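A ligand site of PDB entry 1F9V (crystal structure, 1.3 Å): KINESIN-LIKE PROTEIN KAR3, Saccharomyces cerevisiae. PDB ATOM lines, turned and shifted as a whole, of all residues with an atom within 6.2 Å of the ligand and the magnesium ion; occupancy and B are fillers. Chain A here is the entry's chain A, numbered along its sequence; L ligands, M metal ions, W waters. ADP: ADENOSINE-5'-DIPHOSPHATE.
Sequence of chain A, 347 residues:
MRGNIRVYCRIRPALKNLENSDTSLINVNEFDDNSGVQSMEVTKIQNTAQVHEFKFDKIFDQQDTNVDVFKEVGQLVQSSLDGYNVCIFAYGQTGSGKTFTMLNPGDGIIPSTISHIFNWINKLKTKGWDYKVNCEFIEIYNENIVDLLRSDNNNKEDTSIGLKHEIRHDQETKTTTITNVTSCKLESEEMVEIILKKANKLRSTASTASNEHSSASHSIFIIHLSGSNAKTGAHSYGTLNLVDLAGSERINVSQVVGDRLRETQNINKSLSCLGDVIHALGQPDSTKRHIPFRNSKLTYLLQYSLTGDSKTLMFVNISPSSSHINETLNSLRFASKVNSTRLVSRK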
ATOM      1  N   ARG A  10     -14.875   0.756 -20.128  1.00  0.00           N
ATOM      2  CA  ARG A  10     -13.699   1.415 -19.588  1.00  0.00           C
ATOM      3  C   ARG A  10     -13.373   2.680 -20.349  1.00  0.00           C
ATOM      4  O   ARG A  10     -13.157   2.661 -21.564  1.00  0.00           O
ATOM      5  CB  ARG A  10     -12.471   0.510 -19.612  1.00  0.00           C
ATOM      6  CG  ARG A  10     -11.227   1.230 -19.066  1.00  0.00           C
ATOM      7  CD  ARG A  10      -9.938   0.454 -19.296  1.00  0.00           C
ATOM      8  NE  ARG A  10      -8.890   0.930 -18.390  1.00  0.00           N
ATOM      9  CZ  ARG A  10      -7.734   0.309 -18.204  1.00  0.00           C
ATOM     10  NH1 ARG A  10      -7.453  -0.815 -18.857  1.00  0.00           N
ATOM     11  NH2 ARG A  10      -6.853   0.803 -17.342  1.00  0.00           N
ATOM     12  N   ILE A  11     -13.330   3.796 -19.619  1.00  0.00           N
ATOM     13  CA  ILE A  11     -12.993   5.083 -20.231  1.00  0.00           C
ATOM     14  C   ILE A  11     -11.503   5.283 -19.982  1.00  0.00           C
ATOM     15  O   ILE A  11     -11.055   5.296 -18.832  1.00  0.00           O
ATOM     16  CB  ILE A  11     -13.770   6.249 -19.554  1.00  0.00           C
ATOM     17  CG1 ILE A  11     -15.275   5.998 -19.646  1.00  0.00           C
ATOM     18  CG2 ILE A  11     -13.402   7.573 -20.226  1.00  0.00           C
ATOM     19  CD1 ILE A  11     -16.096   6.773 -18.632  1.00  0.00           C
ATOM     20  N   ARG A  12     -10.718   5.410 -21.041  1.00  0.00           N
ATOM     21  CA  ARG A  12      -9.298   5.625 -20.874  1.00  0.00           C
ATOM     22  C   ARG A  12      -9.027   7.086 -20.572  1.00  0.00           C
ATOM     23  O   ARG A  12      -9.882   7.948 -20.797  1.00  0.00           O
ATOM     24  CB  ARG A  12      -8.549   5.243 -22.162  1.00  0.00           C
ATOM     25  CG  ARG A  12      -8.843   6.144 -23.353  1.00  0.00           C
ATOM     26  CD  ARG A  12      -7.691   6.153 -24.351  1.00  0.00           C
ATOM     27  NE  ARG A  12      -8.041   6.757 -25.646  1.00  0.00           N
ATOM     28  CZ  ARG A  12      -8.131   8.063 -25.867  1.00  0.00           C
ATOM     29  NH1 ARG A  12      -7.899   8.930 -24.881  1.00  0.00           N
ATOM     30  NH2 ARG A  12      -8.457   8.514 -27.072  1.00  0.00           N
ATOM     31  N   PRO A  13      -7.859   7.388 -19.973  1.00  0.00           N
ATOM     32  CA  PRO A  13      -7.535   8.785 -19.679  1.00  0.00           C
ATOM     33  C   PRO A  13      -7.425   9.555 -20.995  1.00  0.00           C
ATOM     34  O   PRO A  13      -7.098   8.979 -22.041  1.00  0.00           O
ATOM     35  CB  PRO A  13      -6.180   8.705 -18.964  1.00  0.00           C
ATOM     36  CG  PRO A  13      -6.089   7.293 -18.462  1.00  0.00           C
ATOM     37  CD  PRO A  13      -6.838   6.455 -19.477  1.00  0.00           C
ATOM     38  N   LEU A  15      -5.797  12.111 -23.730  1.00  0.00           N
ATOM     39  CA  LEU A  15      -4.433  12.482 -24.125  1.00  0.00           C
ATOM     40  C   LEU A  15      -4.433  13.997 -23.889  1.00  0.00           C
ATOM     41  O   LEU A  15      -5.143  14.755 -24.570  1.00  0.00           O
ATOM     42  CB  LEU A  15      -4.159  12.166 -25.593  1.00  0.00           C
ATOM     43  CG  LEU A  15      -3.097  11.098 -25.827  1.00  0.00           C
ATOM     44  CD1 LEU A  15      -2.446  10.673 -24.522  1.00  0.00           C
ATOM     45  CD2 LEU A  15      -3.787   9.969 -26.520  1.00  0.00           C
ATOM     46  N   ASP A  64      -9.087   4.470 -13.102  1.00  0.00           N
ATOM     47  CA  ASP A  64      -8.868   3.030 -13.012  1.00  0.00           C
ATOM     48  C   ASP A  64      -7.705   2.532 -13.850  1.00  0.00           C
ATOM     49  O   ASP A  64      -7.736   2.587 -15.071  1.00  0.00           O
ATOM     50  CB  ASP A  64     -10.146   2.294 -13.418  1.00  0.00           C
ATOM     51  CG  ASP A  64     -11.213   2.356 -12.354  1.00  0.00           C
ATOM     52  OD1 ASP A  64     -10.908   2.086 -11.182  1.00  0.00           O
ATOM     53  OD2 ASP A  64     -12.370   2.693 -12.688  1.00  0.00           O
ATOM     54  N   THR A  65      -6.672   2.049 -13.174  1.00  0.00           N
ATOM     55  CA  THR A  65      -5.479   1.533 -13.829  1.00  0.00           C
ATOM     56  C   THR A  65      -5.691   0.070 -14.247  1.00  0.00           C
ATOM     57  O   THR A  65      -6.708  -0.548 -13.917  1.00  0.00           O
ATOM     58  CB  THR A  65      -4.274   1.566 -12.867  1.00  0.00           C
ATOM     59  OG1 THR A  65      -4.511   0.659 -11.783  1.00  0.00           O
ATOM     60  CG2 THR A  65      -4.062   2.956 -12.303  1.00  0.00           C
ATOM     61  N   ASN A  66      -4.729  -0.491 -14.964  1.00  0.00           N
ATOM     62  CA  ASN A  66      -4.819  -1.883 -15.373  1.00  0.00           C
ATOM     63  C   ASN A  66      -4.882  -2.789 -14.136  1.00  0.00           C
ATOM     64  O   ASN A  66      -5.583  -3.796 -14.139  1.00  0.00           O
ATOM     65  CB  ASN A  66      -3.629  -2.250 -16.249  1.00  0.00           C
ATOM     66  CG  ASN A  66      -3.871  -1.920 -17.703  1.00  0.00           C
ATOM     67  OD1 ASN A  66      -4.862  -1.266 -18.042  1.00  0.00           O
ATOM     68  ND2 ASN A  66      -2.976  -2.359 -18.583  1.00  0.00           N
ATOM     69  N   GLY A  92     -14.041  -1.721 -29.248  1.00  0.00           N
ATOM     70  CA  GLY A  92     -13.983  -0.274 -29.262  1.00  0.00           C
ATOM     71  C   GLY A  92     -13.279   0.261 -30.494  1.00  0.00           C
ATOM     72  O   GLY A  92     -12.619  -0.489 -31.210  1.00  0.00           O
ATOM     73  N   GLN A  93     -13.409   1.557 -30.737  1.00  0.00           N
ATOM     74  CA  GLN A  93     -12.761   2.144 -31.904  1.00  0.00           C
ATOM     75  C   GLN A  93     -11.258   2.146 -31.748  1.00  0.00           C
ATOM     76  O   GLN A  93     -10.737   2.062 -30.636  1.00  0.00           O
ATOM     77  CB  GLN A  93     -13.241   3.589 -32.098  1.00  0.00           C
ATOM     78  CG  GLN A  93     -12.725   4.559 -31.050  1.00  0.00           C
ATOM     79  CD  GLN A  93     -13.107   6.005 -31.345  1.00  0.00           C
ATOM     80  OE1 GLN A  93     -12.824   6.524 -32.428  1.00  0.00           O
ATOM     81  NE2 GLN A  93     -13.747   6.656 -30.389  1.00  0.00           N
ATOM     82  N   THR A  94     -10.557   2.240 -32.866  1.00  0.00           N
ATOM     83  CA  THR A  94      -9.107   2.302 -32.843  1.00  0.00           C
ATOM     84  C   THR A  94      -8.751   3.560 -32.041  1.00  0.00           C
ATOM     85  O   THR A  94      -9.302   4.629 -32.270  1.00  0.00           O
ATOM     86  CB  THR A  94      -8.542   2.380 -34.283  1.00  0.00           C
ATOM     87  OG1 THR A  94      -8.830   1.152 -34.961  1.00  0.00           O
ATOM     88  CG2 THR A  94      -7.041   2.605 -34.265  1.00  0.00           C
ATOM     89  N   GLY A  95      -7.854   3.400 -31.073  1.00  0.00           N
ATOM     90  CA  GLY A  95      -7.449   4.508 -30.234  1.00  0.00           C
ATOM     91  C   GLY A  95      -8.187   4.564 -28.896  1.00  0.00           C
ATOM     92  O   GLY A  95      -7.873   5.403 -28.049  1.00  0.00           O
ATOM     93  N   SER A  96      -9.144   3.661 -28.670  1.00  0.00           N
ATOM     94  CA  SER A  96      -9.891   3.677 -27.420  1.00  0.00           C
ATOM     95  C   SER A  96      -9.198   2.995 -26.244  1.00  0.00           C
ATOM     96  O   SER A  96      -9.550   3.251 -25.085  1.00  0.00           O
ATOM     97  CB  SER A  96     -11.285   3.070 -27.631  1.00  0.00           C
ATOM     98  OG  SER A  96     -11.214   1.705 -28.011  1.00  0.00           O
ATOM     99  N   GLY A  97      -8.227   2.124 -26.520  1.00  0.00           N
ATOM    100  CA  GLY A  97      -7.511   1.433 -25.459  1.00  0.00           C
ATOM    101  C   GLY A  97      -7.596  -0.090 -25.373  1.00  0.00           C
ATOM    102  O   GLY A  97      -7.224  -0.666 -24.345  1.00  0.00           O
ATOM    103  N   LYS A  98      -8.073  -0.757 -26.421  1.00  0.00           N
ATOM    104  CA  LYS A  98      -8.197  -2.221 -26.399  1.00  0.00           C
ATOM    105  C   LYS A  98      -6.864  -2.939 -26.135  1.00  0.00           C
ATOM    106  O   LYS A  98      -6.766  -3.797 -25.253  1.00  0.00           O
ATOM    107  CB  LYS A  98      -8.768  -2.737 -27.731  1.00  0.00           C
ATOM    108  CG  LYS A  98     -10.197  -2.303 -28.001  1.00  0.00           C
ATOM    109  CD  LYS A  98     -10.683  -2.728 -29.376  1.00  0.00           C
ATOM    110  CE  LYS A  98      -9.746  -2.322 -30.499  1.00  0.00           C
ATOM    111  NZ  LYS A  98      -9.794  -0.865 -30.798  1.00  0.00           N
ATOM    112  N   THR A  99      -5.845  -2.596 -26.898  1.00  0.00           N
ATOM    113  CA  THR A  99      -4.536  -3.224 -26.747  1.00  0.00           C
ATOM    114  C   THR A  99      -3.868  -2.886 -25.422  1.00  0.00           C
ATOM    115  O   THR A  99      -3.249  -3.754 -24.806  1.00  0.00           O
ATOM    116  CB  THR A  99      -3.619  -2.837 -27.889  1.00  0.00           C
ATOM    117  OG1 THR A  99      -4.214  -3.268 -29.111  1.00  0.00           O
ATOM    118  CG2 THR A  99      -2.261  -3.506 -27.754  1.00  0.00           C
ATOM    119  N   PHE A 100      -3.996  -1.637 -24.981  1.00  0.00           N
ATOM    120  CA  PHE A 100      -3.403  -1.248 -23.701  1.00  0.00           C
ATOM    121  C   PHE A 100      -4.040  -2.100 -22.603  1.00  0.00           C
ATOM    122  O   PHE A 100      -3.371  -2.601 -21.706  1.00  0.00           O
ATOM    123  CB  PHE A 100      -3.662   0.233 -23.400  1.00  0.00           C
ATOM    124  CG  PHE A 100      -3.016   0.719 -22.131  1.00  0.00           C
ATOM    125  CD1 PHE A 100      -3.633   0.550 -20.902  1.00  0.00           C
ATOM    126  CD2 PHE A 100      -1.764   1.318 -22.175  1.00  0.00           C
ATOM    127  CE1 PHE A 100      -3.026   0.984 -19.715  1.00  0.00           C
ATOM    128  CE2 PHE A 100      -1.136   1.754 -20.995  1.00  0.00           C
ATOM    129  CZ  PHE A 100      -1.774   1.593 -19.769  1.00  0.00           C
ATOM    130  N   THR A 101      -5.351  -2.266 -22.705  1.00  0.00           N
ATOM    131  CA  THR A 101      -6.096  -3.048 -21.735  1.00  0.00           C
ATOM    132  C   THR A 101      -5.705  -4.516 -21.738  1.00  0.00           C
ATOM    133  O   THR A 101      -5.499  -5.109 -20.689  1.00  0.00           O
ATOM    134  CB  THR A 101      -7.609  -2.926 -21.998  1.00  0.00           C
ATOM    135  OG1 THR A 101      -8.037  -1.592 -21.675  1.00  0.00           O
ATOM    136  CG2 THR A 101      -8.393  -3.934 -21.151  1.00  0.00           C
ATOM    137  N   GLU A 212      -2.931   0.779 -38.877  1.00  0.00           N
ATOM    138  CA  GLU A 212      -2.050  -0.369 -38.748  1.00  0.00           C
ATOM    139  C   GLU A 212      -2.793  -1.693 -38.954  1.00  0.00           C
ATOM    140  O   GLU A 212      -4.022  -1.730 -38.906  1.00  0.00           O
ATOM    141  CB  GLU A 212      -1.380  -0.366 -37.374  1.00  0.00           C
ATOM    142  CG  GLU A 212      -2.177  -1.086 -36.307  1.00  0.00           C
ATOM    143  CD  GLU A 212      -1.407  -1.209 -35.008  1.00  0.00           C
ATOM    144  OE1 GLU A 212      -0.172  -0.992 -35.038  1.00  0.00           O
ATOM    145  OE2 GLU A 212      -2.022  -1.510 -33.966  1.00  0.00           O
ATOM    146  N   SER A 214      -2.931  -4.653 -37.070  1.00  0.00           N
ATOM    147  CA  SER A 214      -3.641  -5.202 -35.940  1.00  0.00           C
ATOM    148  C   SER A 214      -4.926  -4.444 -35.649  1.00  0.00           C
ATOM    149  O   SER A 214      -5.840  -4.968 -35.023  1.00  0.00           O
ATOM    150  CB  SER A 214      -2.746  -5.202 -34.699  1.00  0.00           C
ATOM    151  OG  SER A 214      -1.911  -4.057 -34.699  1.00  0.00           O
ATOM    152  N   SER A 215      -5.006  -3.197 -36.104  1.00  0.00           N
ATOM    153  CA  SER A 215      -6.196  -2.395 -35.870  1.00  0.00           C
ATOM    154  C   SER A 215      -7.351  -2.874 -36.757  1.00  0.00           C
ATOM    155  O   SER A 215      -8.514  -2.527 -36.520  1.00  0.00           O
ATOM    156  CB  SER A 215      -5.915  -0.927 -36.143  1.00  0.00           C
ATOM    157  OG  SER A 215      -5.992  -0.645 -37.522  1.00  0.00           O
ATOM    158  N   ASP A 244      -8.512  -9.191 -28.630  1.00  0.00           N
ATOM    159  CA  ASP A 244      -8.306  -7.754 -28.878  1.00  0.00           C
ATOM    160  C   ASP A 244      -8.927  -7.590 -30.275  1.00  0.00           C
ATOM    161  O   ASP A 244      -8.276  -7.821 -31.297  1.00  0.00           O
ATOM    162  CB  ASP A 244      -6.811  -7.466 -28.880  1.00  0.00           C
ATOM    163  CG  ASP A 244      -6.487  -6.008 -29.139  1.00  0.00           C
ATOM    164  OD1 ASP A 244      -7.420  -5.208 -29.381  1.00  0.00           O
ATOM    165  OD2 ASP A 244      -5.288  -5.674 -29.089  1.00  0.00           O
ATOM    166  N   LEU A 245     -10.197  -7.217 -30.296  1.00  0.00           N
ATOM    167  CA  LEU A 245     -10.926  -7.086 -31.556  1.00  0.00           C
ATOM    168  C   LEU A 245     -10.461  -5.987 -32.507  1.00  0.00           C
ATOM    169  O   LEU A 245      -9.744  -5.064 -32.120  1.00  0.00           O
ATOM    170  CB  LEU A 245     -12.420  -6.880 -31.273  1.00  0.00           C
ATOM    171  CG  LEU A 245     -13.163  -7.995 -30.546  1.00  0.00           C
ATOM    172  CD1 LEU A 245     -14.523  -7.477 -30.050  1.00  0.00           C
ATOM    173  CD2 LEU A 245     -13.354  -9.185 -31.477  1.00  0.00           C
ATOM    174  N   ASN A 317     -14.157  -0.479 -24.573  1.00  0.00           N
ATOM    175  CA  ASN A 317     -13.234   0.616 -24.388  1.00  0.00           C
ATOM    176  C   ASN A 317     -13.729   1.857 -25.097  1.00  0.00           C
ATOM    177  O   ASN A 317     -14.157   1.799 -26.251  1.00  0.00           O
ATOM    178  CB  ASN A 317     -11.861   0.255 -24.959  1.00  0.00           C
ATOM    179  CG  ASN A 317     -11.225  -0.903 -24.229  1.00  0.00           C
ATOM    180  OD1 ASN A 317     -11.210  -2.040 -24.707  1.00  0.00           O
ATOM    181  ND2 ASN A 317     -10.689  -0.623 -23.039  1.00  0.00           N
HETATM  182  PB  ADP L   1      -6.633   0.617 -29.416  1.00  0.00           P
HETATM  183  O1B ADP L   1      -8.053   0.555 -28.983  1.00  0.00           O
HETATM  184  O2B ADP L   1      -5.917  -0.809 -29.205  1.00  0.00           O
HETATM  185  O3B ADP L   1      -6.507   1.082 -30.820  1.00  0.00           O
HETATM  186  PA  ADP L   1      -4.428   1.442 -27.739  1.00  0.00           P
HETATM  187  O1A ADP L   1      -4.552   0.561 -26.582  1.00  0.00           O
HETATM  188  O2A ADP L   1      -3.421   0.919 -28.652  1.00  0.00           O
HETATM  189  O3A ADP L   1      -5.825   1.580 -28.471  1.00  0.00           O
HETATM  190  O5' ADP L   1      -3.956   2.893 -27.294  1.00  0.00           O
HETATM  191  C5' ADP L   1      -4.602   4.156 -27.519  1.00  0.00           C
HETATM  192  C4' ADP L   1      -3.650   5.182 -26.838  1.00  0.00           C
HETATM  193  O4' ADP L   1      -4.206   5.432 -25.543  1.00  0.00           O
HETATM  194  C3' ADP L   1      -2.241   4.643 -26.573  1.00  0.00           C
HETATM  195  O3' ADP L   1      -1.222   5.652 -26.720  1.00  0.00           O
HETATM  196  C2' ADP L   1      -2.275   4.114 -25.145  1.00  0.00           C
HETATM  197  O2' ADP L   1      -0.985   4.043 -24.524  1.00  0.00           O
HETATM  198  C1' ADP L   1      -3.292   5.041 -24.492  1.00  0.00           C
HETATM  199  N9  ADP L   1      -4.106   4.357 -23.442  1.00  0.00           N
HETATM  200  C8  ADP L   1      -5.164   3.555 -23.697  1.00  0.00           C
HETATM  201  N7  ADP L   1      -5.690   3.139 -22.564  1.00  0.00           N
HETATM  202  C5  ADP L   1      -5.010   3.653 -21.579  1.00  0.00           C
HETATM  203  C6  ADP L   1      -5.079   3.593 -20.194  1.00  0.00           C
HETATM  204  N6  ADP L   1      -6.041   2.861 -19.606  1.00  0.00           N
HETATM  205  N1  ADP L   1      -4.180   4.269 -19.421  1.00  0.00           N
HETATM  206  C2  ADP L   1      -3.198   5.016 -19.973  1.00  0.00           C
HETATM  207  N3  ADP L   1      -3.115   5.089 -21.316  1.00  0.00           N
HETATM  208  C4  ADP L   1      -3.978   4.433 -22.135  1.00  0.00           C
HETATM  209 MG    MG M   1      -4.825  -1.960 -30.740  1.00  0.00          MG
HETATM  210  O   HOH W   1      -3.034  -0.744 -30.471  1.00  0.00           O
HETATM  211  O   HOH W   2      -4.687   7.626 -23.090  1.00  0.00           O
HETATM  212  O   HOH W   3       0.244   1.657 -25.559  1.00  0.00           O
HETATM  213  O   HOH W   4       0.065   5.290 -22.310  1.00  0.00           O
HETATM  214  O   HOH W   5      -1.403  -0.294 -27.052  1.00  0.00           O
HETATM  215  O   HOH W   6      -4.321   2.893 -31.581  1.00  0.00           O
HETATM  216  O   HOH W   7      -3.538  -3.118 -32.119  1.00  0.00           O
HETATM  217  O   HOH W   8      -5.661  -0.664 -32.437  1.00  0.00           O
HETATM  218  O   HOH W   9      -6.578  -3.314 -30.894  1.00  0.00           O
HETATM  219  O   HOH W  10      -3.869   3.949 -16.779  1.00  0.00           O
HETATM  220  O   HOH W  11      -7.727   1.462 -21.631  1.00  0.00           O
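The side-chain hydroxyl (OG1) of Thr 101 lies within hydrogen-bond range of the backbone carbonyl oxygen (O) of Gly 97 (2.9 Å). The side-chain amide oxygen of Asn 66 lies within hydrogen-bond range of the guanidinium group of Arg 10 (2.8 Å). NH1 of Arg 10 lies within hydrogen-bond range of OG1 of Thr 101 (3.0 Å). The side-chain hydroxyl (OG) of Ser 96 lies within hydrogen-bond range of the backbone carbonyl oxygen (O) of Gln 93. The side-chain amino group of Lys 98 sits at hydrogen-bond distance from the backbone carbonyl oxygen of Gln 93 (3.1 Å). O of Phe 100 lies within hydrogen-bond range of ND2 of Asn 66. The backbone carbonyl oxygen of Asp 64 is in hydrogen-bond range of the guanidinium group of Arg 10, 3.0 Å away. OG1 of Thr 99 sits close to OD2 of Asp 244 (2.6 Å).
The nearest printed residue that does not touch the magnesium ion is Asp 244 (4.1 Å).
The backbone NH (N) of Gly 95 lies within hydrogen-bond range of an oxygen (O3B) of the ligand (2.7 Å). The backbone NH (N) of Lys 98 sits at hydrogen-bond distance from an oxygen (O1B) of the ligand (2.9 Å). The side-chain amino group of Lys 98 lies within salt-bridge range of an oxygen (O1B) of the ligand. An oxygen (O1B) of the ligand is in hydrogen-bond range of the backbone NH (N) of Gly 97. The backbone NH of Thr 99 is in hydrogen-bond range of an oxygen (O1A) of the ligand (3.4 Å). An oxygen (O1A) of the ligand sits at hydrogen-bond distance from the backbone NH (N) of Phe 100 (2.8 Å). The backbone NH (N) of Ser 96 lies within hydrogen-bond range of an oxygen (O1B) of the ligand, 3.3 Å away.
Water W7 lies within hydrogen-bond range of the side-chain carboxylate (OE2) of Glu 212 and the side-chain hydroxyl (OG) of Ser 214. Water W11 lies within hydrogen-bond range of N7 of the ligand (2.8 Å), OG1 of Thr 101 (3.1 Å), NE of Arg 10 (3.5 Å) and O of Gly 97 (3.5 Å). Water W2 bridges the backbone carbonyl oxygen of Pro 13 and an oxygen (O4') of the ligand.
N6 of the ligand sits close to NH2 of Arg 10 (3.2 Å). O of Gln 93 sits close to O1B of the ligand (3.5 Å). Merely in contact with the ligand: Pro 13 (3.4 Å), Thr 94 (3.5 Å) and Arg 12 (3.6 Å). 11 residues have an atom within 4 Å of the ligand: Arg 10, Arg 12, Pro 13, Gln 93, Thr 94, Gly 95, Ser 96, Gly 97, Lys 98, Thr 99 and Phe 100.
The magnesium ion is bound by the side-chain hydroxyl of Thr 99 (2.2 Å), water W1 (2.2 Å), an oxygen (O2B) of the ligand (2.2 Å), water W7 (2.2 Å), water W9 (2.2 Å) and water W8 (2.3 Å).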
